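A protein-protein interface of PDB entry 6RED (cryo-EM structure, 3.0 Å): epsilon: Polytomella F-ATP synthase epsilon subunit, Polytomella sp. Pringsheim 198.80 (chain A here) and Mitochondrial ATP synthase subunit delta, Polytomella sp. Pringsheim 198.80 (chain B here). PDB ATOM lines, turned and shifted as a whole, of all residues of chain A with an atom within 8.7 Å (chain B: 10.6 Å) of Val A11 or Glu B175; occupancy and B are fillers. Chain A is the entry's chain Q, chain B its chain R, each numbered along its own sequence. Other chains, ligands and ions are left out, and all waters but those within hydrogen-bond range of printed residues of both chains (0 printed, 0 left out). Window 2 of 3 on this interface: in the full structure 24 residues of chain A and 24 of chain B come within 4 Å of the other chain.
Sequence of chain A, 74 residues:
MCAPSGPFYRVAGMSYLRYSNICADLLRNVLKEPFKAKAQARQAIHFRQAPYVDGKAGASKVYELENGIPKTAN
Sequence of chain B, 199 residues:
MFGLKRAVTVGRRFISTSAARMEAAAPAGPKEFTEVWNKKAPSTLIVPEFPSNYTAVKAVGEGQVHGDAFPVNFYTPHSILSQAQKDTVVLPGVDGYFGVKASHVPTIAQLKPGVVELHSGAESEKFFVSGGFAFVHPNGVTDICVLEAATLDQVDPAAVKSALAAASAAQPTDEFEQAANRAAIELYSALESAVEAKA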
ATOM      1  N   ALA A   3      -9.491  16.436  -6.947  1.00  0.00           N
ATOM      2  CA  ALA A   3     -10.900  16.530  -7.336  1.00  0.00           C
ATOM      3  C   ALA A   3     -11.715  15.198  -7.370  1.00  0.00           C
ATOM      4  O   ALA A   3     -12.742  15.133  -6.697  1.00  0.00           O
ATOM      5  CB  ALA A   3     -11.016  17.260  -8.688  1.00  0.00           C
ATOM      6  N   PRO A   4     -11.317  14.154  -8.113  1.00  0.00           N
ATOM      7  CA  PRO A   4     -12.240  13.034  -8.307  1.00  0.00           C
ATOM      8  C   PRO A   4     -12.234  12.072  -7.124  1.00  0.00           C
ATOM      9  O   PRO A   4     -11.355  12.091  -6.263  1.00  0.00           O
ATOM     10  CB  PRO A   4     -11.701  12.365  -9.567  1.00  0.00           C
ATOM     11  CG  PRO A   4     -10.253  12.494  -9.416  1.00  0.00           C
ATOM     12  CD  PRO A   4     -10.009  13.816  -8.728  1.00  0.00           C
ATOM     13  N   SER A   5     -13.243  11.212  -7.110  1.00  0.00           N
ATOM     14  CA  SER A   5     -13.447  10.219  -6.070  1.00  0.00           C
ATOM     15  C   SER A   5     -13.200   8.822  -6.627  1.00  0.00           C
ATOM     16  O   SER A   5     -12.803   8.645  -7.780  1.00  0.00           O
ATOM     17  CB  SER A   5     -14.859  10.331  -5.499  1.00  0.00           C
ATOM     18  OG  SER A   5     -15.251   9.119  -4.889  1.00  0.00           O
ATOM     19  N   GLY A   6     -13.435   7.820  -5.786  1.00  0.00           N
ATOM     20  CA  GLY A   6     -13.367   6.447  -6.217  1.00  0.00           C
ATOM     21  C   GLY A   6     -12.343   5.633  -5.456  1.00  0.00           C
ATOM     22  O   GLY A   6     -11.998   5.943  -4.315  1.00  0.00           O
ATOM     23  N   PRO A   7     -11.837   4.566  -6.085  1.00  0.00           N
ATOM     24  CA  PRO A   7     -10.809   3.736  -5.443  1.00  0.00           C
ATOM     25  C   PRO A   7      -9.472   4.443  -5.277  1.00  0.00           C
ATOM     26  O   PRO A   7      -9.309   5.583  -5.715  1.00  0.00           O
ATOM     27  CB  PRO A   7     -10.699   2.539  -6.391  1.00  0.00           C
ATOM     28  CG  PRO A   7     -12.006   2.503  -7.095  1.00  0.00           C
ATOM     29  CD  PRO A   7     -12.378   3.922  -7.291  1.00  0.00           C
ATOM     30  N   PHE A   8      -8.510   3.770  -4.639  1.00  0.00           N
ATOM     31  CA  PHE A   8      -7.300   4.452  -4.188  1.00  0.00           C
ATOM     32  C   PHE A   8      -6.395   4.848  -5.340  1.00  0.00           C
ATOM     33  O   PHE A   8      -5.704   5.868  -5.257  1.00  0.00           O
ATOM     34  CB  PHE A   8      -6.539   3.582  -3.192  1.00  0.00           C
ATOM     35  CG  PHE A   8      -5.955   2.322  -3.774  1.00  0.00           C
ATOM     36  CD1 PHE A   8      -4.631   2.271  -4.170  1.00  0.00           C
ATOM     37  CD2 PHE A   8      -6.719   1.175  -3.876  1.00  0.00           C
ATOM     38  CE1 PHE A   8      -4.094   1.123  -4.681  1.00  0.00           C
ATOM     39  CE2 PHE A   8      -6.179   0.021  -4.387  1.00  0.00           C
ATOM     40  CZ  PHE A   8      -4.865  -0.003  -4.788  1.00  0.00           C
ATOM     41  N   TYR A   9      -6.367   4.056  -6.406  1.00  0.00           N
ATOM     42  CA  TYR A   9      -5.675   4.484  -7.610  1.00  0.00           C
ATOM     43  C   TYR A   9      -6.403   5.642  -8.267  1.00  0.00           C
ATOM     44  O   TYR A   9      -5.764   6.545  -8.813  1.00  0.00           O
ATOM     45  CB  TYR A   9      -5.529   3.315  -8.585  1.00  0.00           C
ATOM     46  CG  TYR A   9      -6.790   2.517  -8.829  1.00  0.00           C
ATOM     47  CD1 TYR A   9      -7.068   1.383  -8.088  1.00  0.00           C
ATOM     48  CD2 TYR A   9      -7.684   2.877  -9.820  1.00  0.00           C
ATOM     49  CE1 TYR A   9      -8.205   0.656  -8.311  1.00  0.00           C
ATOM     50  CE2 TYR A   9      -8.822   2.155 -10.047  1.00  0.00           C
ATOM     51  CZ  TYR A   9      -9.075   1.047  -9.293  1.00  0.00           C
ATOM     52  OH  TYR A   9     -10.212   0.322  -9.523  1.00  0.00           O
ATOM     53  N   ARG A  10      -7.729   5.655  -8.183  1.00  0.00           N
ATOM     54  CA  ARG A  10      -8.508   6.637  -8.917  1.00  0.00           C
ATOM     55  C   ARG A  10      -8.416   8.015  -8.280  1.00  0.00           C
ATOM     56  O   ARG A  10      -8.459   9.025  -8.990  1.00  0.00           O
ATOM     57  CB  ARG A  10      -9.954   6.169  -9.006  1.00  0.00           C
ATOM     58  CG  ARG A  10     -10.803   6.944  -9.973  1.00  0.00           C
ATOM     59  CD  ARG A  10     -10.315   6.767 -11.388  1.00  0.00           C
ATOM     60  NE  ARG A  10     -10.427   5.389 -11.842  1.00  0.00           N
ATOM     61  CZ  ARG A  10     -10.406   5.034 -13.118  1.00  0.00           C
ATOM     62  NH1 ARG A  10     -10.280   5.955 -14.060  1.00  0.00           N
ATOM     63  NH2 ARG A  10     -10.515   3.763 -13.453  1.00  0.00           N
ATOM     64  N   VAL A  11      -8.259   8.085  -6.955  1.00  0.00           N
ATOM     65  CA  VAL A  11      -8.030   9.382  -6.322  1.00  0.00           C
ATOM     66  C   VAL A  11      -6.609   9.871  -6.526  1.00  0.00           C
ATOM     67  O   VAL A  11      -6.326  11.045  -6.262  1.00  0.00           O
ATOM     68  CB  VAL A  11      -8.316   9.380  -4.808  1.00  0.00           C
ATOM     69  CG1 VAL A  11      -9.729   8.907  -4.534  1.00  0.00           C
ATOM     70  CG2 VAL A  11      -7.298   8.551  -4.053  1.00  0.00           C
ATOM     71  N   ALA A  12      -5.709   9.009  -6.980  1.00  0.00           N
ATOM     72  CA  ALA A  12      -4.353   9.408  -7.311  1.00  0.00           C
ATOM     73  C   ALA A  12      -4.224   9.868  -8.749  1.00  0.00           C
ATOM     74  O   ALA A  12      -3.133  10.269  -9.160  1.00  0.00           O
ATOM     75  CB  ALA A  12      -3.383   8.255  -7.052  1.00  0.00           C
ATOM     76  N   GLY A  13      -5.306   9.821  -9.521  1.00  0.00           N
ATOM     77  CA  GLY A  13      -5.241  10.041 -10.948  1.00  0.00           C
ATOM     78  C   GLY A  13      -4.826   8.833 -11.754  1.00  0.00           C
ATOM     79  O   GLY A  13      -4.973   8.847 -12.982  1.00  0.00           O
ATOM     80  N   MET A  14      -4.316   7.793 -11.103  1.00  0.00           N
ATOM     81  CA  MET A  14      -3.931   6.560 -11.766  1.00  0.00           C
ATOM     82  C   MET A  14      -5.175   5.855 -12.287  1.00  0.00           C
ATOM     83  O   MET A  14      -6.129   5.635 -11.542  1.00  0.00           O
ATOM     84  CB  MET A  14      -3.166   5.670 -10.789  1.00  0.00           C
ATOM     85  CG  MET A  14      -2.755   4.335 -11.328  1.00  0.00           C
ATOM     86  SD  MET A  14      -2.088   3.261 -10.050  1.00  0.00           S
ATOM     87  CE  MET A  14      -0.486   3.986  -9.787  1.00  0.00           C
ATOM     88  N   SER A  15      -5.170   5.522 -13.573  1.00  0.00           N
ATOM     89  CA  SER A  15      -6.313   4.890 -14.209  1.00  0.00           C
ATOM     90  C   SER A  15      -6.440   3.442 -13.751  1.00  0.00           C
ATOM     91  O   SER A  15      -5.585   2.911 -13.040  1.00  0.00           O
ATOM     92  CB  SER A  15      -6.167   4.968 -15.721  1.00  0.00           C
ATOM     93  OG  SER A  15      -7.190   4.247 -16.360  1.00  0.00           O
ATOM     94  N   LYS A  71       5.364   3.174 -13.741  1.00  0.00           N
ATOM     95  CA  LYS A  71       4.817   3.314 -12.399  1.00  0.00           C
ATOM     96  C   LYS A  71       4.946   4.722 -11.852  1.00  0.00           C
ATOM     97  O   LYS A  71       4.240   5.068 -10.900  1.00  0.00           O
ATOM     98  CB  LYS A  71       5.504   2.340 -11.446  1.00  0.00           C
ATOM     99  CG  LYS A  71       5.539   0.935 -11.966  1.00  0.00           C
ATOM    100  CD  LYS A  71       6.398   0.051 -11.103  1.00  0.00           C
ATOM    101  CE  LYS A  71       6.770  -1.200 -11.869  1.00  0.00           C
ATOM    102  NZ  LYS A  71       7.359  -0.856 -13.197  1.00  0.00           N
ATOM    103  N   ALA A  73       4.464   8.868 -12.019  1.00  0.00           N
ATOM    104  CA  ALA A  73       3.309   9.659 -12.400  1.00  0.00           C
ATOM    105  C   ALA A  73       3.506  10.283 -13.777  1.00  0.00           C
ATOM    106  O   ALA A  73       4.630  10.500 -14.240  1.00  0.00           O
ATOM    107  CB  ALA A  73       3.045  10.751 -11.368  1.00  0.00           C
ATOM    108  N   ALA B 170      10.512   2.095   0.920  1.00  0.00           N
ATOM    109  CA  ALA B 170      10.576   3.416   0.307  1.00  0.00           C
ATOM    110  C   ALA B 170       9.170   3.938   0.047  1.00  0.00           C
ATOM    111  O   ALA B 170       8.444   3.385  -0.784  1.00  0.00           O
ATOM    112  CB  ALA B 170      11.373   3.358  -0.992  1.00  0.00           C
ATOM    113  N   GLN B 171       8.796   5.015   0.734  1.00  0.00           N
ATOM    114  CA  GLN B 171       7.453   5.593   0.642  1.00  0.00           C
ATOM    115  C   GLN B 171       7.551   7.047   0.199  1.00  0.00           C
ATOM    116  O   GLN B 171       7.645   7.957   1.033  1.00  0.00           O
ATOM    117  CB  GLN B 171       6.706   5.487   1.972  1.00  0.00           C
ATOM    118  CG  GLN B 171       6.151   4.108   2.310  1.00  0.00           C
ATOM    119  CD  GLN B 171       7.220   3.109   2.704  1.00  0.00           C
ATOM    120  OE1 GLN B 171       7.378   2.068   2.064  1.00  0.00           O
ATOM    121  NE2 GLN B 171       7.966   3.417   3.759  1.00  0.00           N
ATOM    122  N   PRO B 172       7.525   7.306  -1.105  1.00  0.00           N
ATOM    123  CA  PRO B 172       7.607   8.686  -1.590  1.00  0.00           C
ATOM    124  C   PRO B 172       6.327   9.466  -1.349  1.00  0.00           C
ATOM    125  O   PRO B 172       5.221   8.920  -1.326  1.00  0.00           O
ATOM    126  CB  PRO B 172       7.864   8.521  -3.094  1.00  0.00           C
ATOM    127  CG  PRO B 172       8.235   7.089  -3.284  1.00  0.00           C
ATOM    128  CD  PRO B 172       7.539   6.336  -2.208  1.00  0.00           C
ATOM    129  N   THR B 173       6.495  10.778  -1.182  1.00  0.00           N
ATOM    130  CA  THR B 173       5.365  11.645  -0.888  1.00  0.00           C
ATOM    131  C   THR B 173       4.487  11.915  -2.098  1.00  0.00           C
ATOM    132  O   THR B 173       3.353  12.380  -1.919  1.00  0.00           O
ATOM    133  CB  THR B 173       5.844  12.971  -0.306  1.00  0.00           C
ATOM    134  OG1 THR B 173       4.706  13.785   0.007  1.00  0.00           O
ATOM    135  CG2 THR B 173       6.746  13.703  -1.291  1.00  0.00           C
ATOM    136  N   ASP B 174       4.973  11.671  -3.312  1.00  0.00           N
ATOM    137  CA  ASP B 174       4.123  11.780  -4.491  1.00  0.00           C
ATOM    138  C   ASP B 174       3.156  10.602  -4.477  1.00  0.00           C
ATOM    139  O   ASP B 174       3.562   9.454  -4.676  1.00  0.00           O
ATOM    140  CB  ASP B 174       4.981  11.812  -5.752  1.00  0.00           C
ATOM    141  CG  ASP B 174       4.218  12.293  -6.984  1.00  0.00           C
ATOM    142  OD1 ASP B 174       4.871  12.563  -8.015  1.00  0.00           O
ATOM    143  OD2 ASP B 174       2.975  12.410  -6.938  1.00  0.00           O
ATOM    144  N   GLU B 175       1.875  10.884  -4.226  1.00  0.00           N
ATOM    145  CA  GLU B 175       0.939   9.840  -3.827  1.00  0.00           C
ATOM    146  C   GLU B 175       0.486   8.957  -4.978  1.00  0.00           C
ATOM    147  O   GLU B 175      -0.142   7.926  -4.728  1.00  0.00           O
ATOM    148  CB  GLU B 175      -0.257  10.459  -3.097  1.00  0.00           C
ATOM    149  CG  GLU B 175      -1.033  11.504  -3.860  1.00  0.00           C
ATOM    150  CD  GLU B 175      -2.241  10.946  -4.555  1.00  0.00           C
ATOM    151  OE1 GLU B 175      -2.664   9.827  -4.204  1.00  0.00           O
ATOM    152  OE2 GLU B 175      -2.790  11.648  -5.427  1.00  0.00           O
ATOM    153  N   PHE B 176       0.801   9.327  -6.219  1.00  0.00           N
ATOM    154  CA  PHE B 176       0.781   8.369  -7.318  1.00  0.00           C
ATOM    155  C   PHE B 176       1.715   7.195  -7.032  1.00  0.00           C
ATOM    156  O   PHE B 176       1.336   6.022  -7.169  1.00  0.00           O
ATOM    157  CB  PHE B 176       1.201   9.089  -8.591  1.00  0.00           C
ATOM    158  CG  PHE B 176       0.650   8.508  -9.844  1.00  0.00           C
ATOM    159  CD1 PHE B 176      -0.413   9.117 -10.485  1.00  0.00           C
ATOM    160  CD2 PHE B 176       1.216   7.380 -10.412  1.00  0.00           C
ATOM    161  CE1 PHE B 176      -0.911   8.604 -11.658  1.00  0.00           C
ATOM    162  CE2 PHE B 176       0.724   6.864 -11.583  1.00  0.00           C
ATOM    163  CZ  PHE B 176      -0.341   7.477 -12.205  1.00  0.00           C
ATOM    164  N   GLU B 177       2.940   7.496  -6.605  1.00  0.00           N
ATOM    165  CA  GLU B 177       3.883   6.443  -6.252  1.00  0.00           C
ATOM    166  C   GLU B 177       3.477   5.711  -4.984  1.00  0.00           C
ATOM    167  O   GLU B 177       3.799   4.532  -4.833  1.00  0.00           O
ATOM    168  CB  GLU B 177       5.291   7.018  -6.112  1.00  0.00           C
ATOM    169  CG  GLU B 177       6.027   7.267  -7.432  1.00  0.00           C
ATOM    170  CD  GLU B 177       5.602   8.535  -8.152  1.00  0.00           C
ATOM    171  OE1 GLU B 177       4.709   9.247  -7.664  1.00  0.00           O
ATOM    172  OE2 GLU B 177       6.179   8.826  -9.218  1.00  0.00           O
ATOM    173  N   GLN B 178       2.747   6.356  -4.076  1.00  0.00           N
ATOM    174  CA  GLN B 178       2.285   5.588  -2.928  1.00  0.00           C
ATOM    175  C   GLN B 178       1.068   4.747  -3.268  1.00  0.00           C
ATOM    176  O   GLN B 178       0.837   3.736  -2.603  1.00  0.00           O
ATOM    177  CB  GLN B 178       1.991   6.489  -1.729  1.00  0.00           C
ATOM    178  CG  GLN B 178       0.566   6.960  -1.575  1.00  0.00           C
ATOM    179  CD  GLN B 178       0.449   8.030  -0.526  1.00  0.00           C
ATOM    180  OE1 GLN B 178       1.440   8.414   0.091  1.00  0.00           O
ATOM    181  NE2 GLN B 178      -0.763   8.517  -0.310  1.00  0.00           N
ATOM    182  N   ALA B 179       0.311   5.118  -4.309  1.00  0.00           N
ATOM    183  CA  ALA B 179      -0.714   4.228  -4.843  1.00  0.00           C
ATOM    184  C   ALA B 179      -0.081   2.985  -5.445  1.00  0.00           C
ATOM    185  O   ALA B 179      -0.544   1.862  -5.206  1.00  0.00           O
ATOM    186  CB  ALA B 179      -1.552   4.960  -5.885  1.00  0.00           C
ATOM    187  N   ALA B 180       0.999   3.176  -6.207  1.00  0.00           N
ATOM    188  CA  ALA B 180       1.751   2.038  -6.727  1.00  0.00           C
ATOM    189  C   ALA B 180       2.372   1.213  -5.607  1.00  0.00           C
ATOM    190  O   ALA B 180       2.419  -0.017  -5.694  1.00  0.00           O
ATOM    191  CB  ALA B 180       2.835   2.510  -7.690  1.00  0.00           C
ATOM    192  N   ASN B 181       2.811   1.866  -4.532  1.00  0.00           N
ATOM    193  CA  ASN B 181       3.371   1.147  -3.396  1.00  0.00           C
ATOM    194  C   ASN B 181       2.304   0.349  -2.660  1.00  0.00           C
ATOM    195  O   ASN B 181       2.578  -0.764  -2.201  1.00  0.00           O
ATOM    196  CB  ASN B 181       4.036   2.130  -2.437  1.00  0.00           C
ATOM    197  CG  ASN B 181       4.913   1.448  -1.415  1.00  0.00           C
ATOM    198  OD1 ASN B 181       5.129   0.246  -1.473  1.00  0.00           O
ATOM    199  ND2 ASN B 181       5.399   2.211  -0.454  1.00  0.00           N
ATOM    200  N   ARG B 182       1.100   0.904  -2.531  1.00  0.00           N
ATOM    201  CA  ARG B 182       0.006   0.185  -1.892  1.00  0.00           C
ATOM    202  C   ARG B 182      -0.379  -1.038  -2.705  1.00  0.00           C
ATOM    203  O   ARG B 182      -0.595  -2.117  -2.143  1.00  0.00           O
ATOM    204  CB  ARG B 182      -1.185   1.121  -1.705  1.00  0.00           C
ATOM    205  CG  ARG B 182      -2.448   0.479  -1.172  1.00  0.00           C
ATOM    206  CD  ARG B 182      -3.480   1.553  -0.844  1.00  0.00           C
ATOM    207  NE  ARG B 182      -4.776   0.998  -0.465  1.00  0.00           N
ATOM    208  CZ  ARG B 182      -5.809   1.722  -0.054  1.00  0.00           C
ATOM    209  NH1 ARG B 182      -5.709   3.037   0.040  1.00  0.00           N
ATOM    210  NH2 ARG B 182      -6.945   1.128   0.268  1.00  0.00           N
ATOM    211  N   ALA B 183      -0.410  -0.897  -4.039  1.00  0.00           N
ATOM    212  CA  ALA B 183      -0.649  -2.040  -4.917  1.00  0.00           C
ATOM    213  C   ALA B 183       0.452  -3.086  -4.783  1.00  0.00           C
ATOM    214  O   ALA B 183       0.175  -4.292  -4.772  1.00  0.00           O
ATOM    215  CB  ALA B 183      -0.755  -1.569  -6.361  1.00  0.00           C
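The side-chain carboxylate of Glu B177 lies within hydrogen-bond range of the backbone NH of Ala A73, at 3.3 Å.
Pro A4 touches none of the printed residues of chain B.
Ser A5 touches none of the printed residues of chain B.
Of the printed residues of chain B, Phe A8 touches Ala B179 (3.7 Å) and Arg B182 (3.4 Å).
Val A11 touches one residue of chain B.
Of chain B, only Glu B175, Phe B176 and Ala B179 come within 4 Å of Ala A12.
Of the printed residues of chain B, Gly A13 touches Phe B176 (3.9 Å).
Printed residues of chain B within 4 Å of Lys A71: Phe B176 (3.8 Å).
Gln B171 touches none of the printed residues of chain A.
Glu B175 touches two residues of chain A.
The nearest residue of chain A that does not touch Glu B175 is Phe A8 (5.1 Å).
Ala B179 touches Phe A8 (O to CE1, 3.7 Å).
Arg B182 touches Phe A8.
Val A11 touches Glu B175 (O to OE2, 3.7 Å).
Ala A12 touches Glu B175.
Ala A12 touches Phe B176.
Ala B179 touches Ala A12 (CB to CB, 3.9 Å).
Gly A13 touches Phe B176.
Phe B176 touches Met A14.
CE of Met A14 touches N of Ala B180, 3.96 Å away.
Phe B176 touches Ala A73 (CG to CB, 3.6 Å).
O of Tyr A9 sits at hydrogen-bond distance from N of Met A14.
Printed residues of chain B that touch a printed residue of chain A: Glu B175, Phe B176, Glu B177, Ala B179, Ala B180 and Arg B182.
Of the 15 printed residues of chain A, 7 touch a printed residue of chain B.
Printed residues of chain A that touch a printed residue of chain B: Phe A8, Val A11, Ala A12, Gly A13, Met A14, Lys A71 and Ala A73.
Among the printed residues, 12 pairs touch across the chains.
Among the printed residues, no Asp or Glu carboxylate lies within 4 Å of a Lys or Arg side-chain nitrogen of the other chain.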
